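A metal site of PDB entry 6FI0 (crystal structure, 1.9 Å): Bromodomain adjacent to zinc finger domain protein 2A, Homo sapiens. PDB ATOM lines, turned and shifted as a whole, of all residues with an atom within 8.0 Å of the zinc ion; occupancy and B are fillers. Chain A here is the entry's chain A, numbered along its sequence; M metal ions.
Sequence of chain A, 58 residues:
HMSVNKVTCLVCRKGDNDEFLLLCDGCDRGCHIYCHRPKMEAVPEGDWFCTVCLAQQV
Within 4 Å of the zinc ion: Cys 24, Cys 27, Cys 50 and Cys 53. The nearest printed residue that does not touch the zinc ion is Gly 26 (4.1 Å).
The zinc ion is bound by SG of Cys 24 (2.2 Å). SG of Cys 27 is bound to the zinc ion (2.3 Å). SG of Cys 50 binds the zinc ion, at 2.3 Å. The side-chain sulfur (SG) of Cys 53 is bound to the zinc ion, at 2.3 Å.
The backbone NH of Gly 26 lies close to the side-chain sulfur of Cys 24 (3.2 Å). N of Cys 24 lies within hydrogen-bond range of O of Arg 29, at 3.0 Å. The side-chain sulfur (SG) of Cys 27 sits close to the guanidinium group (NH1) of Arg 29, 3.3 Å away. SG of Cys 50 sits close to N of Val 52 (3.5 Å).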
ATOM      1  N   LEU A  10      -5.674   1.084   2.493  1.00  0.00           N
ATOM      2  CA  LEU A  10      -5.228   1.724   3.728  1.00  0.00           C
ATOM      3  C   LEU A  10      -5.278   0.824   4.979  1.00  0.00           C
ATOM      4  O   LEU A  10      -4.396   0.913   5.827  1.00  0.00           O
ATOM      5  CB  LEU A  10      -5.992   3.026   4.007  1.00  0.00           C
ATOM      6  CG  LEU A  10      -5.639   4.263   3.203  1.00  0.00           C
ATOM      7  CD1 LEU A  10      -6.670   5.361   3.413  1.00  0.00           C
ATOM      8  CD2 LEU A  10      -4.221   4.780   3.542  1.00  0.00           C
ATOM      9  N   LEU A  23     -11.238   3.930  -4.571  1.00  0.00           N
ATOM     10  CA  LEU A  23     -10.135   4.817  -4.906  1.00  0.00           C
ATOM     11  C   LEU A  23     -10.562   6.236  -4.530  1.00  0.00           C
ATOM     12  O   LEU A  23     -11.660   6.697  -4.932  1.00  0.00           O
ATOM     13  CB  LEU A  23      -9.828   4.720  -6.422  1.00  0.00           C
ATOM     14  CG  LEU A  23      -9.776   3.309  -7.055  1.00  0.00           C
ATOM     15  CD1 LEU A  23      -9.732   3.365  -8.586  1.00  0.00           C
ATOM     16  CD2 LEU A  23      -8.600   2.485  -6.531  1.00  0.00           C
ATOM     17  N   CYS A  24      -9.717   6.931  -3.759  1.00  0.00           N
ATOM     18  CA  CYS A  24     -10.047   8.234  -3.202  1.00  0.00           C
ATOM     19  C   CYS A  24     -10.071   9.217  -4.331  1.00  0.00           C
ATOM     20  O   CYS A  24      -9.202   9.177  -5.212  1.00  0.00           O
ATOM     21  CB  CYS A  24      -9.008   8.709  -2.154  1.00  0.00           C
ATOM     22  SG  CYS A  24      -9.356  10.355  -1.415  1.00  0.00           S
ATOM     23  N   ASP A  25     -11.072  10.093  -4.321  1.00  0.00           N
ATOM     24  CA  ASP A  25     -11.126  11.180  -5.319  1.00  0.00           C
ATOM     25  C   ASP A  25     -10.289  12.433  -4.971  1.00  0.00           C
ATOM     26  O   ASP A  25     -10.114  13.329  -5.788  1.00  0.00           O
ATOM     27  CB  ASP A  25     -12.585  11.482  -5.610  1.00  0.00           C
ATOM     28  CG  ASP A  25     -13.252  10.324  -6.312  1.00  0.00           C
ATOM     29  OD1 ASP A  25     -12.804   9.961  -7.421  1.00  0.00           O
ATOM     30  OD2 ASP A  25     -14.194   9.717  -5.765  1.00  0.00           O
ATOM     31  N   GLY A  26      -9.711  12.481  -3.779  1.00  0.00           N
ATOM     32  CA  GLY A  26      -8.848  13.564  -3.407  1.00  0.00           C
ATOM     33  C   GLY A  26      -7.363  13.254  -3.475  1.00  0.00           C
ATOM     34  O   GLY A  26      -6.554  14.186  -3.412  1.00  0.00           O
ATOM     35  N   CYS A  27      -6.982  11.969  -3.559  1.00  0.00           N
ATOM     36  CA  CYS A  27      -5.555  11.576  -3.574  1.00  0.00           C
ATOM     37  C   CYS A  27      -5.487  10.211  -4.222  1.00  0.00           C
ATOM     38  O   CYS A  27      -6.478   9.765  -4.780  1.00  0.00           O
ATOM     39  CB  CYS A  27      -5.004  11.556  -2.156  1.00  0.00           C
ATOM     40  SG  CYS A  27      -5.678  10.245  -1.115  1.00  0.00           S
ATOM     41  N   ASP A  28      -4.329   9.548  -4.174  1.00  0.00           N
ATOM     42  CA  ASP A  28      -4.183   8.198  -4.749  1.00  0.00           C
ATOM     43  C   ASP A  28      -4.338   7.040  -3.722  1.00  0.00           C
ATOM     44  O   ASP A  28      -3.891   5.919  -3.974  1.00  0.00           O
ATOM     45  CB  ASP A  28      -2.841   8.092  -5.506  1.00  0.00           C
ATOM     46  CG  ASP A  28      -1.623   8.120  -4.587  1.00  0.00           C
ATOM     47  OD1 ASP A  28      -1.713   8.640  -3.439  1.00  0.00           O
ATOM     48  OD2 ASP A  28      -0.556   7.616  -5.021  1.00  0.00           O
ATOM     49  N   ARG A  29      -5.003   7.294  -2.597  1.00  0.00           N
ATOM     50  CA  ARG A  29      -5.129   6.266  -1.565  1.00  0.00           C
ATOM     51  C   ARG A  29      -6.337   5.381  -1.893  1.00  0.00           C
ATOM     52  O   ARG A  29      -7.202   5.761  -2.698  1.00  0.00           O
ATOM     53  CB  ARG A  29      -5.266   6.894  -0.156  1.00  0.00           C
ATOM     54  CG  ARG A  29      -3.969   7.470   0.359  1.00  0.00           C
ATOM     55  CD  ARG A  29      -4.166   8.190   1.675  1.00  0.00           C
ATOM     56  NE  ARG A  29      -2.920   8.797   2.117  1.00  0.00           N
ATOM     57  CZ  ARG A  29      -2.502   9.985   1.762  1.00  0.00           C
ATOM     58  NH1 ARG A  29      -3.203  10.751   0.934  1.00  0.00           N
ATOM     59  NH2 ARG A  29      -1.328  10.434   2.231  1.00  0.00           N
ATOM     60  N   GLY A  30      -6.399   4.206  -1.264  1.00  0.00           N
ATOM     61  CA  GLY A  30      -7.498   3.248  -1.562  1.00  0.00           C
ATOM     62  C   GLY A  30      -7.987   2.491  -0.367  1.00  0.00           C
ATOM     63  O   GLY A  30      -7.389   2.585   0.688  1.00  0.00           O
ATOM     64  N   TRP A  48     -15.846   9.421  -3.361  1.00  0.00           N
ATOM     65  CA  TRP A  48     -15.453   8.915  -2.037  1.00  0.00           C
ATOM     66  C   TRP A  48     -14.084   9.541  -1.637  1.00  0.00           C
ATOM     67  O   TRP A  48     -13.159   9.638  -2.448  1.00  0.00           O
ATOM     68  CB  TRP A  48     -15.407   7.396  -2.013  1.00  0.00           C
ATOM     69  CG  TRP A  48     -14.964   6.873  -0.714  1.00  0.00           C
ATOM     70  CD1 TRP A  48     -15.687   6.770   0.429  1.00  0.00           C
ATOM     71  CD2 TRP A  48     -13.652   6.472  -0.407  1.00  0.00           C
ATOM     72  NE1 TRP A  48     -14.875   6.307   1.451  1.00  0.00           N
ATOM     73  CE2 TRP A  48     -13.629   6.089   0.944  1.00  0.00           C
ATOM     74  CE3 TRP A  48     -12.474   6.381  -1.144  1.00  0.00           C
ATOM     75  CZ2 TRP A  48     -12.481   5.642   1.562  1.00  0.00           C
ATOM     76  CZ3 TRP A  48     -11.342   5.892  -0.539  1.00  0.00           C
ATOM     77  CH2 TRP A  48     -11.353   5.544   0.803  1.00  0.00           C
ATOM     78  N   PHE A  49     -14.036  10.016  -0.384  1.00  0.00           N
ATOM     79  CA  PHE A  49     -12.825  10.557   0.206  1.00  0.00           C
ATOM     80  C   PHE A  49     -12.320   9.714   1.369  1.00  0.00           C
ATOM     81  O   PHE A  49     -13.073   9.351   2.272  1.00  0.00           O
ATOM     82  CB  PHE A  49     -13.026  11.988   0.672  1.00  0.00           C
ATOM     83  CG  PHE A  49     -13.381  12.916  -0.459  1.00  0.00           C
ATOM     84  CD1 PHE A  49     -12.394  13.361  -1.318  1.00  0.00           C
ATOM     85  CD2 PHE A  49     -14.693  13.277  -0.701  1.00  0.00           C
ATOM     86  CE1 PHE A  49     -12.694  14.213  -2.369  1.00  0.00           C
ATOM     87  CE2 PHE A  49     -15.018  14.143  -1.757  1.00  0.00           C
ATOM     88  CZ  PHE A  49     -14.005  14.601  -2.592  1.00  0.00           C
ATOM     89  N   CYS A  50     -11.016   9.493   1.339  1.00  0.00           N
ATOM     90  CA  CYS A  50     -10.298   8.808   2.401  1.00  0.00           C
ATOM     91  C   CYS A  50     -10.183   9.707   3.617  1.00  0.00           C
ATOM     92  O   CYS A  50     -10.525  10.888   3.583  1.00  0.00           O
ATOM     93  CB  CYS A  50      -8.926   8.376   1.901  1.00  0.00           C
ATOM     94  SG  CYS A  50      -7.639   9.653   1.844  1.00  0.00           S
ATOM     95  N   THR A  51      -9.688   9.146   4.695  1.00  0.00           N
ATOM     96  CA  THR A  51      -9.571   9.848   5.960  1.00  0.00           C
ATOM     97  C   THR A  51      -8.531  10.977   5.964  1.00  0.00           C
ATOM     98  O   THR A  51      -8.654  11.969   6.691  1.00  0.00           O
ATOM     99  CB  THR A  51      -9.293   8.811   7.033  1.00  0.00           C
ATOM    100  OG1 THR A  51      -8.316   7.898   6.545  1.00  0.00           O
ATOM    101  CG2 THR A  51     -10.600   8.001   7.298  1.00  0.00           C
ATOM    102  N   VAL A  52      -7.510  10.828   5.149  1.00  0.00           N
ATOM    103  CA  VAL A  52      -6.492  11.846   5.036  1.00  0.00           C
ATOM    104  C   VAL A  52      -7.094  13.083   4.321  1.00  0.00           C
ATOM    105  O   VAL A  52      -6.938  14.211   4.807  1.00  0.00           O
ATOM    106  CB  VAL A  52      -5.264  11.302   4.299  1.00  0.00           C
ATOM    107  CG1 VAL A  52      -4.203  12.384   4.166  1.00  0.00           C
ATOM    108  CG2 VAL A  52      -4.705  10.069   5.036  1.00  0.00           C
ATOM    109  N   CYS A  53      -7.833  12.847   3.240  1.00  0.00           N
ATOM    110  CA  CYS A  53      -8.619  13.902   2.601  1.00  0.00           C
ATOM    111  C   CYS A  53      -9.722  14.502   3.444  1.00  0.00           C
ATOM    112  O   CYS A  53      -9.882  15.738   3.422  1.00  0.00           O
ATOM    113  CB  CYS A  53      -9.196  13.435   1.274  1.00  0.00           C
ATOM    114  SG  CYS A  53      -7.843  13.158   0.089  1.00  0.00           S
ATOM    115  N   LEU A  54     -10.463  13.690   4.199  1.00  0.00           N
ATOM    116  CA  LEU A  54     -11.451  14.255   5.134  1.00  0.00           C
ATOM    117  C   LEU A  54     -10.804  15.228   6.145  1.00  0.00           C
ATOM    118  O   LEU A  54     -11.385  16.267   6.480  1.00  0.00           O
ATOM    119  CB  LEU A  54     -12.177  13.152   5.894  1.00  0.00           C
ATOM    120  CG  LEU A  54     -13.176  12.293   5.108  1.00  0.00           C
ATOM    121  CD1 LEU A  54     -13.655  11.136   5.984  1.00  0.00           C
ATOM    122  CD2 LEU A  54     -14.356  13.126   4.615  1.00  0.00           C
ATOM    123  N   GLN A  56      -8.493  17.299   5.597  1.00  0.00           N
ATOM    124  CA  GLN A  56      -8.173  18.589   4.909  1.00  0.00           C
ATOM    125  C   GLN A  56      -9.388  19.469   4.659  1.00  0.00           C
ATOM    126  O   GLN A  56      -9.250  20.669   4.333  1.00  0.00           O
ATOM    127  CB  GLN A  56      -7.481  18.310   3.572  1.00  0.00           C
ATOM    128  CG  GLN A  56      -6.146  17.614   3.690  1.00  0.00           C
ATOM    129  CD  GLN A  56      -5.089  18.472   4.382  1.00  0.00           C
ATOM    130  OE1 GLN A  56      -4.623  18.119   5.471  1.00  0.00           O
ATOM    131  NE2 GLN A  56      -4.755  19.654   3.784  1.00  0.00           N
HETATM  132 ZN    ZN M   1      -7.622  10.846  -0.127  1.00  0.00          ZN
